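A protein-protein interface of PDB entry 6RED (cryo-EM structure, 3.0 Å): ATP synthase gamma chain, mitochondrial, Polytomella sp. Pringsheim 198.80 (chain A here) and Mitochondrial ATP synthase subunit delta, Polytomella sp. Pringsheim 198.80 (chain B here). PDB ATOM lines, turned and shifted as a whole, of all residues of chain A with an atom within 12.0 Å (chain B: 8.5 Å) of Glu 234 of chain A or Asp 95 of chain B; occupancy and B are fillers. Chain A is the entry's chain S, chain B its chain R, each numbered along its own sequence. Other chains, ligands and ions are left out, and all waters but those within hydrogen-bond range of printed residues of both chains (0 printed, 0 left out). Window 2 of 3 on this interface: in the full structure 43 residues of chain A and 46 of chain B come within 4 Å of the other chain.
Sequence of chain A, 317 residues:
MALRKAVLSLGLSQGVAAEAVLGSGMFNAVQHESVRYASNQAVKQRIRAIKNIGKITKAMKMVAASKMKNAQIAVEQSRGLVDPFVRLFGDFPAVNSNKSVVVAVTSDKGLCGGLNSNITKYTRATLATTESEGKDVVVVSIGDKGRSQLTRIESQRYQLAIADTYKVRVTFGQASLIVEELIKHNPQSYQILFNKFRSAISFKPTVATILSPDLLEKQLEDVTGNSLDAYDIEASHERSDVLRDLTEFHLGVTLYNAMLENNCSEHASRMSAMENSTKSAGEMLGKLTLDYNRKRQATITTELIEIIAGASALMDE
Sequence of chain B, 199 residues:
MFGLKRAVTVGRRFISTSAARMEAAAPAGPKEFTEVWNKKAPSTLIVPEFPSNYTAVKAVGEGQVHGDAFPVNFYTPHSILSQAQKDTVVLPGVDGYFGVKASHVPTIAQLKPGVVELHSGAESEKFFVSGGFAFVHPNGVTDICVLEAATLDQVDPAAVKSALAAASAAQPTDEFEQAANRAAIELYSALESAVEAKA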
ATOM      1  N   LEU A  88     -13.454 -12.260  12.295  1.00  0.00           N
ATOM      2  CA  LEU A  88     -13.656 -11.593  11.015  1.00  0.00           C
ATOM      3  C   LEU A  88     -13.305 -12.495   9.839  1.00  0.00           C
ATOM      4  O   LEU A  88     -14.147 -12.757   8.978  1.00  0.00           O
ATOM      5  CB  LEU A  88     -12.818 -10.313  10.961  1.00  0.00           C
ATOM      6  CG  LEU A  88     -13.085  -9.342   9.824  1.00  0.00           C
ATOM      7  CD1 LEU A  88     -14.136  -8.367  10.249  1.00  0.00           C
ATOM      8  CD2 LEU A  88     -11.827  -8.620   9.476  1.00  0.00           C
ATOM      9  N   LEU A 228     -17.654 -11.114   2.896  1.00  0.00           N
ATOM     10  CA  LEU A 228     -16.991  -9.911   3.356  1.00  0.00           C
ATOM     11  C   LEU A 228     -17.670  -8.651   2.854  1.00  0.00           C
ATOM     12  O   LEU A 228     -17.345  -7.558   3.321  1.00  0.00           O
ATOM     13  CB  LEU A 228     -15.535  -9.930   2.905  1.00  0.00           C
ATOM     14  CG  LEU A 228     -14.485  -9.377   3.852  1.00  0.00           C
ATOM     15  CD1 LEU A 228     -14.707  -9.885   5.264  1.00  0.00           C
ATOM     16  CD2 LEU A 228     -13.140  -9.822   3.347  1.00  0.00           C
ATOM     17  N   ASP A 229     -18.616  -8.781   1.926  1.00  0.00           N
ATOM     18  CA  ASP A 229     -19.313  -7.634   1.376  1.00  0.00           C
ATOM     19  C   ASP A 229     -20.325  -7.044   2.339  1.00  0.00           C
ATOM     20  O   ASP A 229     -20.824  -5.947   2.085  1.00  0.00           O
ATOM     21  CB  ASP A 229     -20.002  -8.026   0.075  1.00  0.00           C
ATOM     22  CG  ASP A 229     -19.022  -8.292  -1.038  1.00  0.00           C
ATOM     23  OD1 ASP A 229     -17.855  -7.870  -0.917  1.00  0.00           O
ATOM     24  OD2 ASP A 229     -19.412  -8.919  -2.039  1.00  0.00           O
ATOM     25  N   ALA A 230     -20.640  -7.736   3.432  1.00  0.00           N
ATOM     26  CA  ALA A 230     -21.489  -7.151   4.458  1.00  0.00           C
ATOM     27  C   ALA A 230     -20.773  -6.066   5.238  1.00  0.00           C
ATOM     28  O   ALA A 230     -21.434  -5.247   5.879  1.00  0.00           O
ATOM     29  CB  ALA A 230     -21.981  -8.229   5.413  1.00  0.00           C
ATOM     30  N   TYR A 231     -19.444  -6.048   5.205  1.00  0.00           N
ATOM     31  CA  TYR A 231     -18.672  -5.019   5.879  1.00  0.00           C
ATOM     32  C   TYR A 231     -18.468  -3.827   4.958  1.00  0.00           C
ATOM     33  O   TYR A 231     -18.087  -3.984   3.798  1.00  0.00           O
ATOM     34  CB  TYR A 231     -17.323  -5.571   6.318  1.00  0.00           C
ATOM     35  CG  TYR A 231     -17.406  -6.693   7.309  1.00  0.00           C
ATOM     36  CD1 TYR A 231     -17.540  -6.441   8.664  1.00  0.00           C
ATOM     37  CD2 TYR A 231     -17.344  -8.005   6.893  1.00  0.00           C
ATOM     38  CE1 TYR A 231     -17.616  -7.469   9.574  1.00  0.00           C
ATOM     39  CE2 TYR A 231     -17.416  -9.035   7.792  1.00  0.00           C
ATOM     40  CZ  TYR A 231     -17.549  -8.762   9.128  1.00  0.00           C
ATOM     41  OH  TYR A 231     -17.619  -9.800  10.011  1.00  0.00           O
ATOM     42  N   ASP A 232     -18.711  -2.637   5.487  1.00  0.00           N
ATOM     43  CA  ASP A 232     -18.568  -1.394   4.743  1.00  0.00           C
ATOM     44  C   ASP A 232     -17.196  -0.815   5.051  1.00  0.00           C
ATOM     45  O   ASP A 232     -16.948  -0.362   6.166  1.00  0.00           O
ATOM     46  CB  ASP A 232     -19.687  -0.429   5.129  1.00  0.00           C
ATOM     47  CG  ASP A 232     -19.664   0.859   4.333  1.00  0.00           C
ATOM     48  OD1 ASP A 232     -19.140   0.872   3.202  1.00  0.00           O
ATOM     49  OD2 ASP A 232     -20.173   1.872   4.851  1.00  0.00           O
ATOM     50  N   ILE A 233     -16.307  -0.823   4.065  1.00  0.00           N
ATOM     51  CA  ILE A 233     -14.918  -0.421   4.276  1.00  0.00           C
ATOM     52  C   ILE A 233     -14.836   1.090   4.430  1.00  0.00           C
ATOM     53  O   ILE A 233     -15.238   1.837   3.534  1.00  0.00           O
ATOM     54  CB  ILE A 233     -14.037  -0.897   3.119  1.00  0.00           C
ATOM     55  CG1 ILE A 233     -14.120  -2.414   2.977  1.00  0.00           C
ATOM     56  CG2 ILE A 233     -12.623  -0.436   3.320  1.00  0.00           C
ATOM     57  CD1 ILE A 233     -13.735  -3.162   4.209  1.00  0.00           C
ATOM     58  N   GLU A 234     -14.287   1.544   5.552  1.00  0.00           N
ATOM     59  CA  GLU A 234     -14.145   2.959   5.859  1.00  0.00           C
ATOM     60  C   GLU A 234     -12.681   3.368   5.887  1.00  0.00           C
ATOM     61  O   GLU A 234     -12.254   4.146   6.735  1.00  0.00           O
ATOM     62  CB  GLU A 234     -14.804   3.293   7.193  1.00  0.00           C
ATOM     63  CG  GLU A 234     -16.326   3.242   7.192  1.00  0.00           C
ATOM     64  CD  GLU A 234     -16.966   4.420   6.466  1.00  0.00           C
ATOM     65  OE1 GLU A 234     -16.415   5.541   6.533  1.00  0.00           O
ATOM     66  OE2 GLU A 234     -18.020   4.220   5.824  1.00  0.00           O
ATOM     67  N   ALA A 235     -11.898   2.853   4.953  1.00  0.00           N
ATOM     68  CA  ALA A 235     -10.474   3.111   4.915  1.00  0.00           C
ATOM     69  C   ALA A 235     -10.117   4.022   3.749  1.00  0.00           C
ATOM     70  O   ALA A 235     -10.982   4.500   3.014  1.00  0.00           O
ATOM     71  CB  ALA A 235      -9.714   1.800   4.835  1.00  0.00           C
ATOM     72  N   SER A 236      -8.817   4.256   3.571  1.00  0.00           N
ATOM     73  CA  SER A 236      -8.344   5.204   2.569  1.00  0.00           C
ATOM     74  C   SER A 236      -8.505   4.655   1.161  1.00  0.00           C
ATOM     75  O   SER A 236      -9.211   5.233   0.330  1.00  0.00           O
ATOM     76  CB  SER A 236      -6.881   5.532   2.822  1.00  0.00           C
ATOM     77  OG  SER A 236      -6.088   4.399   2.537  1.00  0.00           O
ATOM     78  N   HIS A 237      -7.840   3.551   0.871  1.00  0.00           N
ATOM     79  CA  HIS A 237      -7.808   2.982  -0.460  1.00  0.00           C
ATOM     80  C   HIS A 237      -8.746   1.792  -0.544  1.00  0.00           C
ATOM     81  O   HIS A 237      -9.566   1.557   0.342  1.00  0.00           O
ATOM     82  CB  HIS A 237      -6.381   2.611  -0.834  1.00  0.00           C
ATOM     83  CG  HIS A 237      -5.553   3.786  -1.230  1.00  0.00           C
ATOM     84  ND1 HIS A 237      -5.415   4.897  -0.430  1.00  0.00           N
ATOM     85  CD2 HIS A 237      -4.843   4.037  -2.351  1.00  0.00           C
ATOM     86  CE1 HIS A 237      -4.640   5.777  -1.035  1.00  0.00           C
ATOM     87  NE2 HIS A 237      -4.280   5.280  -2.203  1.00  0.00           N
ATOM     88  N   GLU A 238      -8.636   1.041  -1.631  1.00  0.00           N
ATOM     89  CA  GLU A 238      -9.570  -0.031  -1.907  1.00  0.00           C
ATOM     90  C   GLU A 238      -9.323  -1.224  -0.993  1.00  0.00           C
ATOM     91  O   GLU A 238      -8.313  -1.308  -0.295  1.00  0.00           O
ATOM     92  CB  GLU A 238      -9.459  -0.462  -3.363  1.00  0.00           C
ATOM     93  CG  GLU A 238      -8.057  -0.887  -3.748  1.00  0.00           C
ATOM     94  CD  GLU A 238      -7.988  -1.474  -5.142  1.00  0.00           C
ATOM     95  OE1 GLU A 238      -9.053  -1.671  -5.762  1.00  0.00           O
ATOM     96  OE2 GLU A 238      -6.866  -1.718  -5.634  1.00  0.00           O
ATOM     97  N   ARG A 239     -10.271  -2.164  -1.026  1.00  0.00           N
ATOM     98  CA  ARG A 239     -10.262  -3.334  -0.154  1.00  0.00           C
ATOM     99  C   ARG A 239      -9.070  -4.251  -0.383  1.00  0.00           C
ATOM    100  O   ARG A 239      -8.698  -4.993   0.527  1.00  0.00           O
ATOM    101  CB  ARG A 239     -11.551  -4.124  -0.347  1.00  0.00           C
ATOM    102  CG  ARG A 239     -11.942  -4.970   0.825  1.00  0.00           C
ATOM    103  CD  ARG A 239     -13.354  -5.458   0.681  1.00  0.00           C
ATOM    104  NE  ARG A 239     -13.507  -6.415  -0.406  1.00  0.00           N
ATOM    105  CZ  ARG A 239     -14.667  -6.960  -0.749  1.00  0.00           C
ATOM    106  NH1 ARG A 239     -15.769  -6.635  -0.094  1.00  0.00           N
ATOM    107  NH2 ARG A 239     -14.727  -7.827  -1.744  1.00  0.00           N
ATOM    108  N   SER A 240      -8.442  -4.201  -1.556  1.00  0.00           N
ATOM    109  CA  SER A 240      -7.253  -5.009  -1.786  1.00  0.00           C
ATOM    110  C   SER A 240      -6.054  -4.512  -0.994  1.00  0.00           C
ATOM    111  O   SER A 240      -5.061  -5.236  -0.887  1.00  0.00           O
ATOM    112  CB  SER A 240      -6.897  -5.030  -3.268  1.00  0.00           C
ATOM    113  OG  SER A 240      -6.384  -3.778  -3.679  1.00  0.00           O
ATOM    114  N   ASP A 241      -6.108  -3.294  -0.461  1.00  0.00           N
ATOM    115  CA  ASP A 241      -5.091  -2.827   0.464  1.00  0.00           C
ATOM    116  C   ASP A 241      -5.524  -2.904   1.916  1.00  0.00           C
ATOM    117  O   ASP A 241      -4.673  -3.104   2.786  1.00  0.00           O
ATOM    118  CB  ASP A 241      -4.686  -1.394   0.125  1.00  0.00           C
ATOM    119  CG  ASP A 241      -3.704  -1.332  -1.026  1.00  0.00           C
ATOM    120  OD1 ASP A 241      -2.495  -1.533  -0.782  1.00  0.00           O
ATOM    121  OD2 ASP A 241      -4.134  -1.094  -2.175  1.00  0.00           O
ATOM    122  N   VAL A 242      -6.822  -2.774   2.195  1.00  0.00           N
ATOM    123  CA  VAL A 242      -7.323  -2.971   3.552  1.00  0.00           C
ATOM    124  C   VAL A 242      -7.119  -4.407   3.986  1.00  0.00           C
ATOM    125  O   VAL A 242      -6.711  -4.675   5.118  1.00  0.00           O
ATOM    126  CB  VAL A 242      -8.803  -2.581   3.638  1.00  0.00           C
ATOM    127  CG1 VAL A 242      -9.256  -2.537   5.077  1.00  0.00           C
ATOM    128  CG2 VAL A 242      -9.002  -1.267   2.972  1.00  0.00           C
ATOM    129  N   LEU A 243      -7.367  -5.350   3.084  1.00  0.00           N
ATOM    130  CA  LEU A 243      -7.147  -6.747   3.412  1.00  0.00           C
ATOM    131  C   LEU A 243      -5.669  -7.080   3.457  1.00  0.00           C
ATOM    132  O   LEU A 243      -5.268  -7.965   4.211  1.00  0.00           O
ATOM    133  CB  LEU A 243      -7.869  -7.634   2.414  1.00  0.00           C
ATOM    134  CG  LEU A 243      -9.185  -8.220   2.910  1.00  0.00           C
ATOM    135  CD1 LEU A 243     -10.161  -7.163   3.363  1.00  0.00           C
ATOM    136  CD2 LEU A 243      -9.788  -9.034   1.803  1.00  0.00           C
ATOM    137  N   ASP A 245      -3.289  -4.934   4.620  1.00  0.00           N
ATOM    138  CA  ASP A 245      -2.916  -4.446   5.941  1.00  0.00           C
ATOM    139  C   ASP A 245      -3.481  -5.332   7.035  1.00  0.00           C
ATOM    140  O   ASP A 245      -2.806  -5.606   8.031  1.00  0.00           O
ATOM    141  CB  ASP A 245      -3.417  -3.021   6.126  1.00  0.00           C
ATOM    142  CG  ASP A 245      -2.850  -2.070   5.106  1.00  0.00           C
ATOM    143  OD1 ASP A 245      -1.760  -2.351   4.570  1.00  0.00           O
ATOM    144  OD2 ASP A 245      -3.499  -1.038   4.843  1.00  0.00           O
ATOM    145  N   LEU A 246      -4.692  -5.843   6.836  1.00  0.00           N
ATOM    146  CA  LEU A 246      -5.323  -6.659   7.858  1.00  0.00           C
ATOM    147  C   LEU A 246      -4.679  -8.031   7.968  1.00  0.00           C
ATOM    148  O   LEU A 246      -4.525  -8.546   9.073  1.00  0.00           O
ATOM    149  CB  LEU A 246      -6.810  -6.791   7.567  1.00  0.00           C
ATOM    150  CG  LEU A 246      -7.741  -5.856   8.312  1.00  0.00           C
ATOM    151  CD1 LEU A 246      -9.145  -6.317   8.107  1.00  0.00           C
ATOM    152  CD2 LEU A 246      -7.407  -5.845   9.771  1.00  0.00           C
ATOM    153  N   LEU B  91     -14.843   6.472  17.206  1.00  0.00           N
ATOM    154  CA  LEU B  91     -13.571   5.953  16.762  1.00  0.00           C
ATOM    155  C   LEU B  91     -12.951   6.856  15.712  1.00  0.00           C
ATOM    156  O   LEU B  91     -13.645   7.299  14.799  1.00  0.00           O
ATOM    157  CB  LEU B  91     -13.746   4.553  16.177  1.00  0.00           C
ATOM    158  CG  LEU B  91     -14.428   3.561  17.103  1.00  0.00           C
ATOM    159  CD1 LEU B  91     -14.926   2.380  16.327  1.00  0.00           C
ATOM    160  CD2 LEU B  91     -13.449   3.138  18.137  1.00  0.00           C
ATOM    161  N   PRO B  92     -11.675   7.121  15.780  1.00  0.00           N
ATOM    162  CA  PRO B  92     -11.052   8.020  14.804  1.00  0.00           C
ATOM    163  C   PRO B  92     -10.671   7.359  13.482  1.00  0.00           C
ATOM    164  O   PRO B  92      -9.521   7.032  13.218  1.00  0.00           O
ATOM    165  CB  PRO B  92      -9.809   8.498  15.549  1.00  0.00           C
ATOM    166  CG  PRO B  92      -9.453   7.357  16.412  1.00  0.00           C
ATOM    167  CD  PRO B  92     -10.726   6.711  16.821  1.00  0.00           C
ATOM    168  N   GLY B  93     -11.650   7.190  12.606  1.00  0.00           N
ATOM    169  CA  GLY B  93     -11.399   6.579  11.318  1.00  0.00           C
ATOM    170  C   GLY B  93     -10.556   7.455  10.418  1.00  0.00           C
ATOM    171  O   GLY B  93     -10.246   8.600  10.730  1.00  0.00           O
ATOM    172  N   VAL B  94     -10.156   6.892   9.280  1.00  0.00           N
ATOM    173  CA  VAL B  94      -9.350   7.661   8.340  1.00  0.00           C
ATOM    174  C   VAL B  94     -10.179   8.765   7.703  1.00  0.00           C
ATOM    175  O   VAL B  94      -9.661   9.842   7.383  1.00  0.00           O
ATOM    176  CB  VAL B  94      -8.724   6.729   7.291  1.00  0.00           C
ATOM    177  CG1 VAL B  94      -7.659   7.450   6.507  1.00  0.00           C
ATOM    178  CG2 VAL B  94      -8.104   5.558   7.968  1.00  0.00           C
ATOM    179  N   ASP B  95     -11.480   8.550   7.554  1.00  0.00           N
ATOM    180  CA  ASP B  95     -12.379   9.579   7.066  1.00  0.00           C
ATOM    181  C   ASP B  95     -12.964  10.429   8.184  1.00  0.00           C
ATOM    182  O   ASP B  95     -14.029  11.019   7.999  1.00  0.00           O
ATOM    183  CB  ASP B  95     -13.508   8.948   6.253  1.00  0.00           C
ATOM    184  CG  ASP B  95     -13.021   8.328   4.964  1.00  0.00           C
ATOM    185  OD1 ASP B  95     -11.980   8.772   4.445  1.00  0.00           O
ATOM    186  OD2 ASP B  95     -13.692   7.410   4.455  1.00  0.00           O
ATOM    187  N   GLY B  96     -12.309  10.493   9.332  1.00  0.00           N
ATOM    188  CA  GLY B  96     -12.788  11.267  10.460  1.00  0.00           C
ATOM    189  C   GLY B  96     -13.446  10.383  11.504  1.00  0.00           C
ATOM    190  O   GLY B  96     -13.570   9.170  11.346  1.00  0.00           O
ATOM    191  N   TYR B  97     -13.870  11.027  12.587  1.00  0.00           N
ATOM    192  CA  TYR B  97     -14.498  10.320  13.690  1.00  0.00           C
ATOM    193  C   TYR B  97     -15.853   9.781  13.273  1.00  0.00           C
ATOM    194  O   TYR B  97     -16.491  10.299  12.360  1.00  0.00           O
ATOM    195  CB  TYR B  97     -14.678  11.238  14.890  1.00  0.00           C
ATOM    196  CG  TYR B  97     -13.414  11.515  15.652  1.00  0.00           C
ATOM    197  CD1 TYR B  97     -12.476  12.408  15.169  1.00  0.00           C
ATOM    198  CD2 TYR B  97     -13.164  10.896  16.861  1.00  0.00           C
ATOM    199  CE1 TYR B  97     -11.324  12.660  15.857  1.00  0.00           C
ATOM    200  CE2 TYR B  97     -12.016  11.148  17.558  1.00  0.00           C
ATOM    201  CZ  TYR B  97     -11.103  12.030  17.049  1.00  0.00           C
ATOM    202  OH  TYR B  97      -9.947  12.289  17.739  1.00  0.00           O
ATOM    203  N   PHE B  98     -16.288   8.722  13.943  1.00  0.00           N
ATOM    204  CA  PHE B  98     -17.607   8.171  13.696  1.00  0.00           C
ATOM    205  C   PHE B  98     -18.051   7.393  14.920  1.00  0.00           C
ATOM    206  O   PHE B  98     -17.255   6.689  15.543  1.00  0.00           O
ATOM    207  CB  PHE B  98     -17.640   7.294  12.436  1.00  0.00           C
ATOM    208  CG  PHE B  98     -16.973   5.969  12.581  1.00  0.00           C
ATOM    209  CD1 PHE B  98     -15.600   5.862  12.617  1.00  0.00           C
ATOM    210  CD2 PHE B  98     -17.726   4.820  12.643  1.00  0.00           C
ATOM    211  CE1 PHE B  98     -15.003   4.639  12.741  1.00  0.00           C
ATOM    212  CE2 PHE B  98     -17.127   3.597  12.764  1.00  0.00           C
ATOM    213  CZ  PHE B  98     -15.772   3.509  12.822  1.00  0.00           C
ATOM    214  N   HIS B 104     -24.735  -0.801  14.662  1.00  0.00           N
ATOM    215  CA  HIS B 104     -24.151  -0.109  13.526  1.00  0.00           C
ATOM    216  C   HIS B 104     -24.243  -0.994  12.287  1.00  0.00           C
ATOM    217  O   HIS B 104     -24.546  -2.186  12.359  1.00  0.00           O
ATOM    218  CB  HIS B 104     -22.697   0.226  13.837  1.00  0.00           C
ATOM    219  CG  HIS B 104     -22.122   1.359  13.049  1.00  0.00           C
ATOM    220  ND1 HIS B 104     -22.204   2.667  13.464  1.00  0.00           N
ATOM    221  CD2 HIS B 104     -21.376   1.372  11.922  1.00  0.00           C
ATOM    222  CE1 HIS B 104     -21.574   3.441  12.602  1.00  0.00           C
ATOM    223  NE2 HIS B 104     -21.063   2.679  11.654  1.00  0.00           N
ATOM    224  N   VAL B 105     -23.996  -0.398  11.133  1.00  0.00           N
ATOM    225  CA  VAL B 105     -23.775  -1.224   9.943  1.00  0.00           C
ATOM    226  C   VAL B 105     -22.446  -1.952  10.109  1.00  0.00           C
ATOM    227  O   VAL B 105     -21.551  -1.423  10.784  1.00  0.00           O
ATOM    228  CB  VAL B 105     -23.803  -0.346   8.681  1.00  0.00           C
ATOM    229  CG1 VAL B 105     -22.735   0.725   8.706  1.00  0.00           C
ATOM    230  CG2 VAL B 105     -23.711  -1.160   7.401  1.00  0.00           C
ATOM    231  N   PRO B 106     -22.309  -3.199   9.656  1.00  0.00           N
ATOM    232  CA  PRO B 106     -21.007  -3.868   9.743  1.00  0.00           C
ATOM    233  C   PRO B 106     -19.945  -3.133   8.943  1.00  0.00           C
ATOM    234  O   PRO B 106     -20.159  -2.764   7.790  1.00  0.00           O
ATOM    235  CB  PRO B 106     -21.294  -5.250   9.163  1.00  0.00           C
ATOM    236  CG  PRO B 106     -22.697  -5.478   9.473  1.00  0.00           C
ATOM    237  CD  PRO B 106     -23.392  -4.163   9.422  1.00  0.00           C
ATOM    238  N   THR B 107     -18.804  -2.894   9.577  1.00  0.00           N
ATOM    239  CA  THR B 107     -17.775  -2.098   8.936  1.00  0.00           C
ATOM    240  C   THR B 107     -16.407  -2.634   9.328  1.00  0.00           C
ATOM    241  O   THR B 107     -16.259  -3.346  10.321  1.00  0.00           O
ATOM    242  CB  THR B 107     -17.919  -0.607   9.296  1.00  0.00           C
ATOM    243  OG1 THR B 107     -17.155   0.181   8.384  1.00  0.00           O
ATOM    244  CG2 THR B 107     -17.402  -0.311  10.675  1.00  0.00           C
ATOM    245  N   ILE B 108     -15.425  -2.342   8.492  1.00  0.00           N
ATOM    246  CA  ILE B 108     -14.021  -2.550   8.797  1.00  0.00           C
ATOM    247  C   ILE B 108     -13.389  -1.187   8.592  1.00  0.00           C
ATOM    248  O   ILE B 108     -13.075  -0.801   7.465  1.00  0.00           O
ATOM    249  CB  ILE B 108     -13.367  -3.608   7.908  1.00  0.00           C
ATOM    250  CG1 ILE B 108     -14.061  -4.952   8.066  1.00  0.00           C
ATOM    251  CG2 ILE B 108     -11.909  -3.752   8.238  1.00  0.00           C
ATOM    252  CD1 ILE B 108     -13.653  -5.939   7.029  1.00  0.00           C
ATOM    253  N   ALA B 109     -13.239  -0.440   9.667  1.00  0.00           N
ATOM    254  CA  ALA B 109     -12.820   0.947   9.597  1.00  0.00           C
ATOM    255  C   ALA B 109     -11.376   1.031  10.037  1.00  0.00           C
ATOM    256  O   ALA B 109     -11.067   0.761  11.199  1.00  0.00           O
ATOM    257  CB  ALA B 109     -13.703   1.815  10.479  1.00  0.00           C
ATOM    258  N   GLN B 110     -10.492   1.379   9.114  1.00  0.00           N
ATOM    259  CA  GLN B 110      -9.123   1.677   9.487  1.00  0.00           C
ATOM    260  C   GLN B 110      -9.116   2.932  10.337  1.00  0.00           C
ATOM    261  O   GLN B 110      -9.901   3.846  10.098  1.00  0.00           O
ATOM    262  CB  GLN B 110      -8.267   1.862   8.245  1.00  0.00           C
ATOM    263  CG  GLN B 110      -6.806   2.005   8.523  1.00  0.00           C
ATOM    264  CD  GLN B 110      -5.978   1.897   7.281  1.00  0.00           C
ATOM    265  OE1 GLN B 110      -6.450   1.437   6.247  1.00  0.00           O
ATOM    266  NE2 GLN B 110      -4.730   2.322   7.370  1.00  0.00           N
ATOM    267  N   LEU B 111      -8.287   2.955  11.368  1.00  0.00           N
ATOM    268  CA  LEU B 111      -8.244   4.091  12.267  1.00  0.00           C
ATOM    269  C   LEU B 111      -6.979   4.894  12.044  1.00  0.00           C
ATOM    270  O   LEU B 111      -5.937   4.354  11.680  1.00  0.00           O
ATOM    271  CB  LEU B 111      -8.324   3.661  13.725  1.00  0.00           C
ATOM    272  CG  LEU B 111      -9.537   2.856  14.159  1.00  0.00           C
ATOM    273  CD1 LEU B 111      -9.506   2.663  15.643  1.00  0.00           C
ATOM    274  CD2 LEU B 111     -10.793   3.549  13.755  1.00  0.00           C
ATOM    275  N   LYS B 112      -7.102   6.189  12.216  1.00  0.00           N
ATOM    276  CA  LYS B 112      -5.980   7.104  12.252  1.00  0.00           C
ATOM    277  C   LYS B 112      -5.717   7.474  13.698  1.00  0.00           C
ATOM    278  O   LYS B 112      -6.526   7.139  14.564  1.00  0.00           O
ATOM    279  CB  LYS B 112      -6.295   8.313  11.373  1.00  0.00           C
ATOM    280  CG  LYS B 112      -7.252   9.305  11.953  1.00  0.00           C
ATOM    281  CD  LYS B 112      -7.463  10.414  10.953  1.00  0.00           C
ATOM    282  CE  LYS B 112      -8.389  11.474  11.485  1.00  0.00           C
ATOM    283  NZ  LYS B 112      -8.547  12.576  10.497  1.00  0.00           N
ATOM    284  N   PHE B 133      -7.214  -0.760  13.465  1.00  0.00           N
ATOM    285  CA  PHE B 133      -8.487  -0.936  12.787  1.00  0.00           C
ATOM    286  C   PHE B 133      -9.598  -0.981  13.817  1.00  0.00           C
ATOM    287  O   PHE B 133      -9.361  -0.894  15.018  1.00  0.00           O
ATOM    288  CB  PHE B 133      -8.500  -2.215  11.962  1.00  0.00           C
ATOM    289  CG  PHE B 133      -7.569  -2.195  10.804  1.00  0.00           C
ATOM    290  CD1 PHE B 133      -8.000  -1.772   9.564  1.00  0.00           C
ATOM    291  CD2 PHE B 133      -6.264  -2.605  10.948  1.00  0.00           C
ATOM    292  CE1 PHE B 133      -7.141  -1.753   8.499  1.00  0.00           C
ATOM    293  CE2 PHE B 133      -5.412  -2.589   9.889  1.00  0.00           C
ATOM    294  CZ  PHE B 133      -5.847  -2.164   8.663  1.00  0.00           C
ATOM    295  N   ALA B 134     -10.821  -1.141  13.332  1.00  0.00           N
ATOM    296  CA  ALA B 134     -11.981  -1.265  14.202  1.00  0.00           C
ATOM    297  C   ALA B 134     -13.082  -1.943  13.414  1.00  0.00           C
ATOM    298  O   ALA B 134     -13.588  -1.365  12.453  1.00  0.00           O
ATOM    299  CB  ALA B 134     -12.452   0.091  14.704  1.00  0.00           C
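The backbone NH (N) of Asp 232 of chain A sits at hydrogen-bond distance from the backbone carbonyl oxygen (O) of Pro 106 of chain B. N of Ile 108 of chain B is in hydrogen-bond range of O of Asp 232 of chain A. O of Ile 108 of chain B is in hydrogen-bond range of N of Glu 234 of chain A, at 3.3 Å. The backbone carbonyl oxygen of Ala 230 of chain A sits close to the backbone carbonyl oxygen of Pro 106 of chain B (3.4 Å). The side-chain hydroxyl of Thr 107 of chain B sits close to the backbone carbonyl oxygen of Asp 232 of chain A (2.3 Å).
O of Gln 110 of chain B lies within hydrogen-bond range of N of Val 94 of chain B. The backbone carbonyl oxygen (O) of Ala 109 of chain B sits at hydrogen-bond distance from the backbone NH (N) of Ala 134 of chain B, 2.9 Å away.
Among the printed residues, merely in contact across the chains: Tyr 231 of chain A with Pro 106 of chain B (3.3 Å), Glu 234 of chain A with Thr 107 of chain B (3.4 Å), Ala 235 of chain A with Gln 110 of chain B (3.6 Å), Asp 245 of chain A with Phe 133 of chain B (3.6 Å), Leu 246 of chain A with Phe 133 of chain B (3.6 Å), Ile 233 of chain A with Ile 108 of chain B (3.7 Å), Tyr 231 of chain A with Thr 107 of chain B (3.7 Å), Tyr 231 of chain A with Ile 108 of chain B (3.8 Å), Glu 234 of chain A with Ala 109 of chain B (3.8 Å), Leu 246 of chain A with Ile 108 of chain B (3.8 Å) and Glu 234 of chain A with Asp 95 of chain B (3.9 Å).
No residue of chain A comes within 4 Å of Val 94 of chain B. No residue of chain A comes within 4 Å of Gly 96 of chain B. Ile 108 of chain B touches just these residues of chain A: Tyr 231 (3.8 Å), Asp 232 (3.4 Å), Ile 233 (3.7 Å), Glu 234 (3.3 Å) and Leu 246 (3.8 Å). Of the printed residues of chain B, Ile 233 of chain A touches Ile 108. Of the printed residues of chain A, Phe 133 of chain B touches Asp 245 (3.6 Å) and Leu 246 (3.6 Å). Asp 241 of chain A touches none of the printed residues of chain B. The nearest residue of chain A that does not touch Asp 95 of chain B is Ala 235 of chain A (4.2 Å). The nearest printed residue of chain B that does not touch Ala 230 of chain A is Val 105 of chain B (4.9 Å).
Of the 19 printed residues of chain A, 8 touch a printed residue of chain B. Printed residues of chain A that touch a printed residue of chain B: Ala 230, Tyr 231, Asp 232, Ile 233, Glu 234, Ala 235, Asp 245 and Leu 246. Hydrophobic or aromatic side chains of chain A within 4 Å of the printed part of chain B: Tyr 231, Ile 233, Ala 235 and Leu 246. Hydrophobic or aromatic side chains of chain B within 4 Å of the printed part of chain A: Pro 106, Ile 108, Ala 109 and Phe 133.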
